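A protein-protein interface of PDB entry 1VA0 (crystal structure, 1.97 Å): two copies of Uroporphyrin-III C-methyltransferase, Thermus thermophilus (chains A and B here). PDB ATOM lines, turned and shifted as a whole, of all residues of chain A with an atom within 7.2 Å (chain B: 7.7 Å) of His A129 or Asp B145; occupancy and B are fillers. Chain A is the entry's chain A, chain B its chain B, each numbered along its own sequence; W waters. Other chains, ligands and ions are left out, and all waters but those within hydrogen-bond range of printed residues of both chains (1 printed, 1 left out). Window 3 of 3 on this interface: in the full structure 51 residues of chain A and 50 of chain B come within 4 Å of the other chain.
Water W1 lies within hydrogen-bond range of the side-chain carboxylate of Glu B139 (2.7 Å) and the backbone NH of Arg A125 (2.8 Å).
The backbone carbonyl oxygen (O) of Val B137 sits at hydrogen-bond distance from the side-chain hydroxyl (OG) of Ser B135 (2.6 Å).
O of Val B134 lies within hydrogen-bond range of N of Leu B158, 2.9 Å away.
The backbone NH (N) of Arg B147 is in hydrogen-bond range of the side-chain carboxylate (OD1) of Asp B145, at 3.3 Å.
Among the printed residues, merely in contact across the chains: Gly A130 with Ala B133 (2.9 Å), Val A152 with Pro B148 (3.4 Å), His A129 with Leu B138 (3.4 Å), Val A152 with Phe B149 (3.5 Å), Arg A125 with Glu B139 (3.5 Å), His A129 with Phe B89 (3.5 Å), His A129 with Phe B149 (3.7 Å), His A129 with Pro B144 (3.7 Å), Gly A130 with Phe B149 (3.7 Å), His A129 with Val B134 (3.7 Å), Phe A131 with Phe B149 (3.8 Å), Pro A153 with Phe B149 (3.8 Å), Phe A131 with Phe B89 (3.8 Å) and Gly A130 with Val B134 (3.97 Å).
No position is printed for both chains.
Of the 18 pairs that touch across the chains among the printed residues, none has its exchanged pair printed and touching as well.
Of the printed residues of chain B, His A129 touches Phe B89, Val B134, Ser B135, Leu B138, Pro B144, Asp B145 and Phe B149.
Of chain A, only His A129 (3.0 Å) comes within 4 Å of Asp B145.
Printed residues of chain B within 4 Å of Arg A125: Glu B139 (3.5 Å).
Printed residues of chain A within 4 Å of Pro B148: Val A152.
Printed residues of chain A within 4 Å of Ala B133: Gly A130 (2.9 Å) and Phe A131 (2.8 Å).
Gly A126 touches none of the printed residues of chain B.
The nearest residue of chain A that does not touch Asp B145 is Pro A153 (6.5 Å).
The nearest printed residue of chain A that does not touch Val B134 is Phe A131 (5.1 Å).
Of the 13 printed residues of chain A, 7 touch a printed residue of chain B.
Printed residues of chain A that touch a printed residue of chain B: Thr A123, Arg A125, His A129, Gly A130, Phe A131, Val A152 and Pro A153.
Hydrophobic or aromatic side chains of chain A within 4 Å of the printed part of chain B: His A129, Phe A131, Val A152 and Pro A153.
Printed residues of chain B that touch a printed residue of chain A: Phe B89, Ala B133, Val B134, Ser B135, Leu B138, Glu B139, Pro B144, Asp B145, Pro B148 and Phe B149.
Hydrophobic or aromatic side chains of chain B that line the printed part of chain A: Phe B89, Val B134, Leu B138, Pro B144, Pro B148 and Phe B149.
The backbone NH (N) of Phe B89 is in hydrogen-bond range of the side-chain hydroxyl (OG1) of Thr A123 (2.8 Å).
The backbone carbonyl oxygen of Phe A131 lies within hydrogen-bond range of the backbone NH of Ala B133.
The backbone NH (N) of Ser B135 lies within hydrogen-bond range of the backbone carbonyl oxygen (O) of His A129 (3.2 Å).
NE2 of His A129 sits at hydrogen-bond distance from O of Asp B145 (3.0 Å).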
ATOM      1  N   LEU A 122       1.835  -6.510 -33.137  1.00  0.00           N
ATOM      2  CA  LEU A 122       2.895  -7.157 -32.353  1.00  0.00           C
ATOM      3  C   LEU A 122       3.862  -6.107 -31.822  1.00  0.00           C
ATOM      4  O   LEU A 122       4.593  -6.333 -30.859  1.00  0.00           O
ATOM      5  CB  LEU A 122       3.626  -8.206 -33.197  1.00  0.00           C
ATOM      6  CG  LEU A 122       2.668  -9.278 -33.729  1.00  0.00           C
ATOM      7  CD1 LEU A 122       3.432 -10.352 -34.495  1.00  0.00           C
ATOM      8  CD2 LEU A 122       1.922  -9.908 -32.551  1.00  0.00           C
ATOM      9  N   THR A 123       3.872  -4.950 -32.468  1.00  0.00           N
ATOM     10  CA  THR A 123       4.702  -3.846 -32.014  1.00  0.00           C
ATOM     11  C   THR A 123       3.697  -2.712 -31.819  1.00  0.00           C
ATOM     12  O   THR A 123       2.713  -2.613 -32.555  1.00  0.00           O
ATOM     13  CB  THR A 123       5.762  -3.433 -33.056  1.00  0.00           C
ATOM     14  OG1 THR A 123       5.125  -3.102 -34.299  1.00  0.00           O
ATOM     15  CG2 THR A 123       6.747  -4.589 -33.280  1.00  0.00           C
ATOM     16  N   HIS A 124       3.921  -1.879 -30.816  1.00  0.00           N
ATOM     17  CA  HIS A 124       3.009  -0.775 -30.570  1.00  0.00           C
ATOM     18  C   HIS A 124       3.664   0.234 -29.662  1.00  0.00           C
ATOM     19  O   HIS A 124       4.296  -0.126 -28.668  1.00  0.00           O
ATOM     20  CB  HIS A 124       1.713  -1.277 -29.931  1.00  0.00           C
ATOM     21  CG  HIS A 124       0.675  -0.211 -29.769  1.00  0.00           C
ATOM     22  ND1 HIS A 124       0.080   0.415 -30.842  1.00  0.00           N
ATOM     23  CD2 HIS A 124       0.145   0.357 -28.660  1.00  0.00           C
ATOM     24  CE1 HIS A 124      -0.771   1.324 -30.402  1.00  0.00           C
ATOM     25  NE2 HIS A 124      -0.751   1.309 -29.081  1.00  0.00           N
ATOM     26  N   ARG A 125       3.506   1.501 -30.020  1.00  0.00           N
ATOM     27  CA  ARG A 125       4.079   2.604 -29.270  1.00  0.00           C
ATOM     28  C   ARG A 125       3.927   2.399 -27.773  1.00  0.00           C
ATOM     29  O   ARG A 125       2.856   2.060 -27.287  1.00  0.00           O
ATOM     30  CB  ARG A 125       3.395   3.909 -29.670  1.00  0.00           C
ATOM     31  CG  ARG A 125       4.162   5.133 -29.254  1.00  0.00           C
ATOM     32  CD  ARG A 125       3.397   6.417 -29.549  1.00  0.00           C
ATOM     33  NE  ARG A 125       4.215   7.576 -29.210  1.00  0.00           N
ATOM     34  CZ  ARG A 125       4.761   7.780 -28.013  1.00  0.00           C
ATOM     35  NH1 ARG A 125       4.574   6.904 -27.029  1.00  0.00           N
ATOM     36  NH2 ARG A 125       5.505   8.858 -27.801  1.00  0.00           N
ATOM     37  N   GLY A 126       5.021   2.589 -27.051  1.00  0.00           N
ATOM     38  CA  GLY A 126       4.995   2.438 -25.611  1.00  0.00           C
ATOM     39  C   GLY A 126       4.917   1.023 -25.063  1.00  0.00           C
ATOM     40  O   GLY A 126       5.225   0.830 -23.898  1.00  0.00           O
ATOM     41  N   LEU A 127       4.517   0.041 -25.873  1.00  0.00           N
ATOM     42  CA  LEU A 127       4.400  -1.338 -25.384  1.00  0.00           C
ATOM     43  C   LEU A 127       5.468  -2.313 -25.888  1.00  0.00           C
ATOM     44  O   LEU A 127       6.033  -3.080 -25.108  1.00  0.00           O
ATOM     45  CB  LEU A 127       3.017  -1.902 -25.729  1.00  0.00           C
ATOM     46  CG  LEU A 127       1.815  -1.115 -25.201  1.00  0.00           C
ATOM     47  CD1 LEU A 127       0.545  -1.825 -25.622  1.00  0.00           C
ATOM     48  CD2 LEU A 127       1.884  -0.993 -23.668  1.00  0.00           C
ATOM     49  N   ALA A 128       5.742  -2.293 -27.188  1.00  0.00           N
ATOM     50  CA  ALA A 128       6.741  -3.201 -27.755  1.00  0.00           C
ATOM     51  C   ALA A 128       7.355  -2.590 -28.997  1.00  0.00           C
ATOM     52  O   ALA A 128       6.634  -2.167 -29.900  1.00  0.00           O
ATOM     53  CB  ALA A 128       6.100  -4.519 -28.112  1.00  0.00           C
ATOM     54  N   HIS A 129       8.684  -2.551 -29.035  1.00  0.00           N
ATOM     55  CA  HIS A 129       9.402  -2.001 -30.170  1.00  0.00           C
ATOM     56  C   HIS A 129       9.966  -3.094 -31.083  1.00  0.00           C
ATOM     57  O   HIS A 129      10.707  -2.802 -32.033  1.00  0.00           O
ATOM     58  CB  HIS A 129      10.523  -1.091 -29.661  1.00  0.00           C
ATOM     59  CG  HIS A 129      11.395  -1.726 -28.619  1.00  0.00           C
ATOM     60  ND1 HIS A 129      10.889  -2.407 -27.528  1.00  0.00           N
ATOM     61  CD2 HIS A 129      12.742  -1.718 -28.463  1.00  0.00           C
ATOM     62  CE1 HIS A 129      11.886  -2.781 -26.743  1.00  0.00           C
ATOM     63  NE2 HIS A 129      13.019  -2.373 -27.287  1.00  0.00           N
ATOM     64  N   GLY A 130       9.617  -4.343 -30.778  1.00  0.00           N
ATOM     65  CA  GLY A 130      10.051  -5.472 -31.586  1.00  0.00           C
ATOM     66  C   GLY A 130       9.370  -6.684 -31.000  1.00  0.00           C
ATOM     67  O   GLY A 130       8.662  -6.558 -30.007  1.00  0.00           O
ATOM     68  N   PHE A 131       9.549  -7.853 -31.599  1.00  0.00           N
ATOM     69  CA  PHE A 131       8.928  -9.043 -31.047  1.00  0.00           C
ATOM     70  C   PHE A 131       9.829 -10.237 -31.327  1.00  0.00           C
ATOM     71  O   PHE A 131      10.810 -10.121 -32.064  1.00  0.00           O
ATOM     72  CB  PHE A 131       7.548  -9.270 -31.682  1.00  0.00           C
ATOM     73  CG  PHE A 131       7.600  -9.620 -33.147  1.00  0.00           C
ATOM     74  CD1 PHE A 131       7.650  -8.623 -34.124  1.00  0.00           C
ATOM     75  CD2 PHE A 131       7.602 -10.948 -33.548  1.00  0.00           C
ATOM     76  CE1 PHE A 131       7.697  -8.952 -35.482  1.00  0.00           C
ATOM     77  CE2 PHE A 131       7.651 -11.291 -34.908  1.00  0.00           C
ATOM     78  CZ  PHE A 131       7.698 -10.287 -35.873  1.00  0.00           C
ATOM     79  N   VAL A 152      11.663 -10.648 -24.266  1.00  0.00           N
ATOM     80  CA  VAL A 152      11.264  -9.798 -25.368  1.00  0.00           C
ATOM     81  C   VAL A 152       9.861  -9.277 -25.056  1.00  0.00           C
ATOM     82  O   VAL A 152       8.986 -10.050 -24.678  1.00  0.00           O
ATOM     83  CB  VAL A 152      11.298 -10.588 -26.692  1.00  0.00           C
ATOM     84  CG1 VAL A 152      10.786  -9.729 -27.833  1.00  0.00           C
ATOM     85  CG2 VAL A 152      12.745 -11.016 -26.973  1.00  0.00           C
ATOM     86  N   PRO A 153       9.637  -7.959 -25.205  1.00  0.00           N
ATOM     87  CA  PRO A 153       8.350  -7.316 -24.928  1.00  0.00           C
ATOM     88  C   PRO A 153       7.132  -8.054 -25.451  1.00  0.00           C
ATOM     89  O   PRO A 153       6.140  -8.187 -24.750  1.00  0.00           O
ATOM     90  CB  PRO A 153       8.515  -5.935 -25.556  1.00  0.00           C
ATOM     91  CG  PRO A 153       9.971  -5.669 -25.376  1.00  0.00           C
ATOM     92  CD  PRO A 153      10.595  -6.984 -25.761  1.00  0.00           C
ATOM     93  N   THR A 154       7.193  -8.505 -26.701  1.00  0.00           N
ATOM     94  CA  THR A 154       6.092  -9.263 -27.283  1.00  0.00           C
ATOM     95  C   THR A 154       6.692 -10.584 -27.740  1.00  0.00           C
ATOM     96  O   THR A 154       7.656 -10.596 -28.513  1.00  0.00           O
ATOM     97  CB  THR A 154       5.486  -8.557 -28.509  1.00  0.00           C
ATOM     98  OG1 THR A 154       4.868  -7.335 -28.106  1.00  0.00           O
ATOM     99  CG2 THR A 154       4.455  -9.435 -29.180  1.00  0.00           C
ATOM    100  N   PHE B  89       5.796  -2.885 -36.993  1.00  0.00           N
ATOM    101  CA  PHE B  89       6.693  -1.804 -37.399  1.00  0.00           C
ATOM    102  C   PHE B  89       6.093  -0.727 -38.292  1.00  0.00           C
ATOM    103  O   PHE B  89       6.813  -0.126 -39.094  1.00  0.00           O
ATOM    104  CB  PHE B  89       7.915  -2.413 -38.111  1.00  0.00           C
ATOM    105  CG  PHE B  89       8.667  -3.411 -37.268  1.00  0.00           C
ATOM    106  CD1 PHE B  89       9.333  -3.000 -36.113  1.00  0.00           C
ATOM    107  CD2 PHE B  89       8.658  -4.770 -37.594  1.00  0.00           C
ATOM    108  CE1 PHE B  89       9.975  -3.931 -35.280  1.00  0.00           C
ATOM    109  CE2 PHE B  89       9.291  -5.702 -36.772  1.00  0.00           C
ATOM    110  CZ  PHE B  89       9.947  -5.278 -35.612  1.00  0.00           C
ATOM    111  N   ALA B 133      12.702  -9.553 -34.001  1.00  0.00           N
ATOM    112  CA  ALA B 133      12.790  -8.435 -34.935  1.00  0.00           C
ATOM    113  C   ALA B 133      12.643  -7.174 -34.086  1.00  0.00           C
ATOM    114  O   ALA B 133      11.824  -7.135 -33.169  1.00  0.00           O
ATOM    115  CB  ALA B 133      11.677  -8.525 -35.977  1.00  0.00           C
ATOM    116  N   VAL B 134      13.452  -6.160 -34.376  1.00  0.00           N
ATOM    117  CA  VAL B 134      13.422  -4.931 -33.604  1.00  0.00           C
ATOM    118  C   VAL B 134      13.661  -3.734 -34.508  1.00  0.00           C
ATOM    119  O   VAL B 134      14.233  -3.872 -35.595  1.00  0.00           O
ATOM    120  CB  VAL B 134      14.489  -4.974 -32.466  1.00  0.00           C
ATOM    121  CG1 VAL B 134      15.906  -4.901 -33.048  1.00  0.00           C
ATOM    122  CG2 VAL B 134      14.235  -3.851 -31.467  1.00  0.00           C
ATOM    123  N   SER B 135      13.186  -2.567 -34.080  1.00  0.00           N
ATOM    124  CA  SER B 135      13.358  -1.338 -34.856  1.00  0.00           C
ATOM    125  C   SER B 135      14.494  -0.491 -34.279  1.00  0.00           C
ATOM    126  O   SER B 135      14.639  -0.381 -33.051  1.00  0.00           O
ATOM    127  CB  SER B 135      12.058  -0.515 -34.830  1.00  0.00           C
ATOM    128  OG  SER B 135      12.214   0.703 -35.553  1.00  0.00           O
ATOM    129  N   GLY B 136      15.285   0.116 -35.160  1.00  0.00           N
ATOM    130  CA  GLY B 136      16.383   0.966 -34.725  1.00  0.00           C
ATOM    131  C   GLY B 136      15.895   2.373 -34.386  1.00  0.00           C
ATOM    132  O   GLY B 136      16.638   3.196 -33.835  1.00  0.00           O
ATOM    133  N   VAL B 137      14.638   2.654 -34.718  1.00  0.00           N
ATOM    134  CA  VAL B 137      14.044   3.961 -34.450  1.00  0.00           C
ATOM    135  C   VAL B 137      12.645   3.762 -33.858  1.00  0.00           C
ATOM    136  O   VAL B 137      11.821   3.031 -34.395  1.00  0.00           O
ATOM    137  CB  VAL B 137      13.933   4.827 -35.743  1.00  0.00           C
ATOM    138  CG1 VAL B 137      13.294   6.180 -35.412  1.00  0.00           C
ATOM    139  CG2 VAL B 137      15.323   5.048 -36.368  1.00  0.00           C
ATOM    140  N   LEU B 138      12.389   4.413 -32.732  1.00  0.00           N
ATOM    141  CA  LEU B 138      11.096   4.283 -32.082  1.00  0.00           C
ATOM    142  C   LEU B 138      10.214   5.452 -32.491  1.00  0.00           C
ATOM    143  O   LEU B 138      10.689   6.415 -33.097  1.00  0.00           O
ATOM    144  CB  LEU B 138      11.269   4.305 -30.565  1.00  0.00           C
ATOM    145  CG  LEU B 138      12.237   3.279 -29.968  1.00  0.00           C
ATOM    146  CD1 LEU B 138      12.125   3.291 -28.461  1.00  0.00           C
ATOM    147  CD2 LEU B 138      11.930   1.910 -30.513  1.00  0.00           C
ATOM    148  N   GLU B 139       8.922   5.346 -32.197  1.00  0.00           N
ATOM    149  CA  GLU B 139       8.013   6.448 -32.454  1.00  0.00           C
ATOM    150  C   GLU B 139       8.580   7.555 -31.552  1.00  0.00           C
ATOM    151  O   GLU B 139       8.881   7.317 -30.382  1.00  0.00           O
ATOM    152  CB  GLU B 139       6.597   6.087 -31.998  1.00  0.00           C
ATOM    153  CG  GLU B 139       5.973   4.932 -32.754  1.00  0.00           C
ATOM    154  CD  GLU B 139       6.336   3.571 -32.173  1.00  0.00           C
ATOM    155  OE1 GLU B 139       7.276   3.481 -31.346  1.00  0.00           O
ATOM    156  OE2 GLU B 139       5.675   2.583 -32.552  1.00  0.00           O
ATOM    157  N   GLY B 142      13.382   8.040 -30.670  1.00  0.00           N
ATOM    158  CA  GLY B 142      14.340   7.444 -29.753  1.00  0.00           C
ATOM    159  C   GLY B 142      15.021   6.151 -30.198  1.00  0.00           C
ATOM    160  O   GLY B 142      14.715   5.588 -31.252  1.00  0.00           O
ATOM    161  N   TYR B 143      15.955   5.692 -29.371  1.00  0.00           N
ATOM    162  CA  TYR B 143      16.730   4.479 -29.607  1.00  0.00           C
ATOM    163  C   TYR B 143      16.105   3.271 -28.922  1.00  0.00           C
ATOM    164  O   TYR B 143      15.580   3.371 -27.818  1.00  0.00           O
ATOM    165  CB  TYR B 143      18.165   4.657 -29.086  1.00  0.00           C
ATOM    166  CG  TYR B 143      19.046   5.498 -29.981  1.00  0.00           C
ATOM    167  CD1 TYR B 143      18.872   6.881 -30.080  1.00  0.00           C
ATOM    168  CD2 TYR B 143      20.043   4.904 -30.752  1.00  0.00           C
ATOM    169  CE1 TYR B 143      19.667   7.643 -30.928  1.00  0.00           C
ATOM    170  CE2 TYR B 143      20.841   5.652 -31.597  1.00  0.00           C
ATOM    171  CZ  TYR B 143      20.646   7.019 -31.684  1.00  0.00           C
ATOM    172  OH  TYR B 143      21.412   7.751 -32.551  1.00  0.00           O
ATOM    173  N   PRO B 144      16.188   2.094 -29.557  1.00  0.00           N
ATOM    174  CA  PRO B 144      15.607   0.889 -28.962  1.00  0.00           C
ATOM    175  C   PRO B 144      16.422   0.306 -27.820  1.00  0.00           C
ATOM    176  O   PRO B 144      17.648   0.454 -27.764  1.00  0.00           O
ATOM    177  CB  PRO B 144      15.576  -0.079 -30.120  1.00  0.00           C
ATOM    178  CG  PRO B 144      16.897   0.235 -30.802  1.00  0.00           C
ATOM    179  CD  PRO B 144      16.871   1.769 -30.824  1.00  0.00           C
ATOM    180  N   ASP B 145      15.729  -0.345 -26.899  1.00  0.00           N
ATOM    181  CA  ASP B 145      16.413  -1.025 -25.811  1.00  0.00           C
ATOM    182  C   ASP B 145      16.708  -2.391 -26.425  1.00  0.00           C
ATOM    183  O   ASP B 145      15.791  -3.182 -26.636  1.00  0.00           O
ATOM    184  CB  ASP B 145      15.496  -1.209 -24.603  1.00  0.00           C
ATOM    185  CG  ASP B 145      16.178  -1.986 -23.480  1.00  0.00           C
ATOM    186  OD1 ASP B 145      17.395  -2.260 -23.565  1.00  0.00           O
ATOM    187  OD2 ASP B 145      15.494  -2.330 -22.507  1.00  0.00           O
ATOM    188  N   LEU B 146      17.980  -2.666 -26.706  1.00  0.00           N
ATOM    189  CA  LEU B 146      18.369  -3.928 -27.350  1.00  0.00           C
ATOM    190  C   LEU B 146      18.654  -5.117 -26.445  1.00  0.00           C
ATOM    191  O   LEU B 146      18.861  -6.226 -26.917  1.00  0.00           O
ATOM    192  CB  LEU B 146      19.593  -3.686 -28.237  1.00  0.00           C
ATOM    193  CG  LEU B 146      19.302  -2.682 -29.355  1.00  0.00           C
ATOM    194  CD1 LEU B 146      20.592  -2.340 -30.127  1.00  0.00           C
ATOM    195  CD2 LEU B 146      18.234  -3.280 -30.281  1.00  0.00           C
ATOM    196  N   ARG B 147      18.666  -4.894 -25.139  1.00  0.00           N
ATOM    197  CA  ARG B 147      18.970  -5.963 -24.182  1.00  0.00           C
ATOM    198  C   ARG B 147      18.077  -7.211 -24.259  1.00  0.00           C
ATOM    199  O   ARG B 147      18.569  -8.334 -24.205  1.00  0.00           O
ATOM    200  CB  ARG B 147      18.961  -5.389 -22.758  1.00  0.00           C
ATOM    201  CG  ARG B 147      19.157  -6.430 -21.674  1.00  0.00           C
ATOM    202  CD  ARG B 147      19.166  -5.767 -20.328  1.00  0.00           C
ATOM    203  NE  ARG B 147      20.510  -5.286 -20.050  1.00  0.00           N
ATOM    204  CZ  ARG B 147      21.541  -6.106 -19.887  1.00  0.00           C
ATOM    205  NH1 ARG B 147      21.347  -7.418 -19.962  1.00  0.00           N
ATOM    206  NH2 ARG B 147      22.756  -5.628 -19.656  1.00  0.00           N
ATOM    207  N   PRO B 148      16.756  -7.041 -24.394  1.00  0.00           N
ATOM    208  CA  PRO B 148      15.943  -8.262 -24.472  1.00  0.00           C
ATOM    209  C   PRO B 148      16.176  -9.004 -25.805  1.00  0.00           C
ATOM    210  O   PRO B 148      15.850 -10.182 -25.927  1.00  0.00           O
ATOM    211  CB  PRO B 148      14.505  -7.748 -24.373  1.00  0.00           C
ATOM    212  CG  PRO B 148      14.623  -6.324 -23.875  1.00  0.00           C
ATOM    213  CD  PRO B 148      15.915  -5.835 -24.450  1.00  0.00           C
ATOM    214  N   PHE B 149      16.769  -8.317 -26.780  1.00  0.00           N
ATOM    215  CA  PHE B 149      16.991  -8.887 -28.107  1.00  0.00           C
ATOM    216  C   PHE B 149      18.409  -9.318 -28.421  1.00  0.00           C
ATOM    217  O   PHE B 149      18.635 -10.062 -29.376  1.00  0.00           O
ATOM    218  CB  PHE B 149      16.617  -7.859 -29.187  1.00  0.00           C
ATOM    219  CG  PHE B 149      15.199  -7.410 -29.137  1.00  0.00           C
ATOM    220  CD1 PHE B 149      14.207  -8.131 -29.791  1.00  0.00           C
ATOM    221  CD2 PHE B 149      14.847  -6.261 -28.436  1.00  0.00           C
ATOM    222  CE1 PHE B 149      12.882  -7.711 -29.746  1.00  0.00           C
ATOM    223  CE2 PHE B 149      13.522  -5.835 -28.389  1.00  0.00           C
ATOM    224  CZ  PHE B 149      12.537  -6.569 -29.050  1.00  0.00           C
ATOM    225  N   ALA B 150      19.363  -8.842 -27.637  1.00  0.00           N
ATOM    226  CA  ALA B 150      20.762  -9.100 -27.934  1.00  0.00           C
ATOM    227  C   ALA B 150      21.240 -10.511 -28.208  1.00  0.00           C
ATOM    228  O   ALA B 150      22.150 -10.688 -29.014  1.00  0.00           O
ATOM    229  CB  ALA B 150      21.629  -8.478 -26.865  1.00  0.00           C
ATOM    230  N   LEU B 158      14.991  -3.583 -38.379  1.00  0.00           N
ATOM    231  CA  LEU B 158      14.373  -2.701 -39.367  1.00  0.00           C
ATOM    232  C   LEU B 158      14.691  -1.284 -38.920  1.00  0.00           C
ATOM    233  O   LEU B 158      14.885  -1.043 -37.723  1.00  0.00           O
ATOM    234  CB  LEU B 158      12.853  -2.918 -39.448  1.00  0.00           C
ATOM    235  CG  LEU B 158      12.442  -4.266 -40.057  1.00  0.00           C
ATOM    236  CD1 LEU B 158      10.980  -4.214 -40.481  1.00  0.00           C
ATOM    237  CD2 LEU B 158      13.298  -4.571 -41.275  1.00  0.00           C
ATOM    238  N   MET B 159      14.792  -0.366 -39.882  1.00  0.00           N
ATOM    239  CA  MET B 159      15.141   1.019 -39.603  1.00  0.00           C
ATOM    240  C   MET B 159      16.417   1.112 -38.771  1.00  0.00           C
ATOM    241  O   MET B 159      16.480   1.894 -37.817  1.00  0.00           O
ATOM    242  CB  MET B 159      13.974   1.703 -38.884  1.00  0.00           C
ATOM    243  CG  MET B 159      12.692   1.583 -39.697  1.00  0.00           C
ATOM    244  SD  MET B 159      11.207   2.320 -38.977  1.00  0.00           S
ATOM    245  CE  MET B 159      10.474   0.886 -38.111  1.00  0.00           C
ATOM    246  N   TRP B 166      26.000   2.402 -34.063  1.00  0.00           N
ATOM    247  CA  TRP B 166      25.579   2.371 -32.669  1.00  0.00           C
ATOM    248  C   TRP B 166      24.924   1.034 -32.334  1.00  0.00           C
ATOM    249  O   TRP B 166      25.184   0.463 -31.283  1.00  0.00           O
ATOM    250  CB  TRP B 166      24.574   3.489 -32.379  1.00  0.00           C
ATOM    251  CG  TRP B 166      24.116   3.503 -30.933  1.00  0.00           C
ATOM    252  CD1 TRP B 166      24.696   4.173 -29.901  1.00  0.00           C
ATOM    253  CD2 TRP B 166      22.996   2.796 -30.376  1.00  0.00           C
ATOM    254  NE1 TRP B 166      24.004   3.934 -28.732  1.00  0.00           N
ATOM    255  CE2 TRP B 166      22.957   3.094 -28.996  1.00  0.00           C
ATOM    256  CE3 TRP B 166      22.018   1.944 -30.912  1.00  0.00           C
ATOM    257  CZ2 TRP B 166      21.980   2.565 -28.136  1.00  0.00           C
ATOM    258  CZ3 TRP B 166      21.040   1.417 -30.055  1.00  0.00           C
ATOM    259  CH2 TRP B 166      21.031   1.734 -28.682  1.00  0.00           C
ATOM    260  N   GLU B 170      26.369  -1.607 -29.677  1.00  0.00           N
ATOM    261  CA  GLU B 170      25.544  -1.967 -28.536  1.00  0.00           C
ATOM    262  C   GLU B 170      25.372  -3.494 -28.469  1.00  0.00           C
ATOM    263  O   GLU B 170      25.481  -4.078 -27.398  1.00  0.00           O
ATOM    264  CB  GLU B 170      24.200  -1.246 -28.629  1.00  0.00           C
ATOM    265  CG  GLU B 170      23.252  -1.486 -27.469  1.00  0.00           C
ATOM    266  CD  GLU B 170      23.773  -0.986 -26.116  1.00  0.00           C
ATOM    267  OE1 GLU B 170      24.911  -0.474 -26.026  1.00  0.00           O
ATOM    268  OE2 GLU B 170      23.024  -1.119 -25.125  1.00  0.00           O
ATOM    269  N   ARG B 173      28.461  -4.954 -27.180  1.00  0.00           N
ATOM    270  CA  ARG B 173      28.519  -4.702 -25.739  1.00  0.00           C
ATOM    271  C   ARG B 173      27.618  -5.690 -25.004  1.00  0.00           C
ATOM    272  O   ARG B 173      27.898  -6.091 -23.876  1.00  0.00           O
ATOM    273  CB  ARG B 173      28.045  -3.278 -25.413  1.00  0.00           C
ATOM    274  CG  ARG B 173      28.097  -2.951 -23.923  1.00  0.00           C
ATOM    275  CD  ARG B 173      27.600  -1.538 -23.620  1.00  0.00           C
ATOM    276  NE  ARG B 173      26.140  -1.435 -23.588  1.00  0.00           N
ATOM    277  CZ  ARG B 173      25.361  -1.945 -22.638  1.00  0.00           C
ATOM    278  NH1 ARG B 173      25.889  -2.612 -21.617  1.00  0.00           N
ATOM    279  NH2 ARG B 173      24.046  -1.777 -22.703  1.00  0.00           N
ATOM    280  N   LEU B 174      26.521  -6.076 -25.642  1.00  0.00           N
ATOM    281  CA  LEU B 174      25.592  -6.992 -25.005  1.00  0.00           C
ATOM    282  C   LEU B 174      25.927  -8.473 -25.242  1.00  0.00           C
ATOM    283  O   LEU B 174      25.128  -9.365 -24.928  1.00  0.00           O
ATOM    284  CB  LEU B 174      24.164  -6.654 -25.444  1.00  0.00           C
ATOM    285  CG  LEU B 174      23.646  -5.317 -24.884  1.00  0.00           C
ATOM    286  CD1 LEU B 174      22.432  -4.878 -25.670  1.00  0.00           C
ATOM    287  CD2 LEU B 174      23.303  -5.445 -23.383  1.00  0.00           C
HETATM  288  O   HOH W   1       3.006   2.182 -32.737  1.00  0.00           O
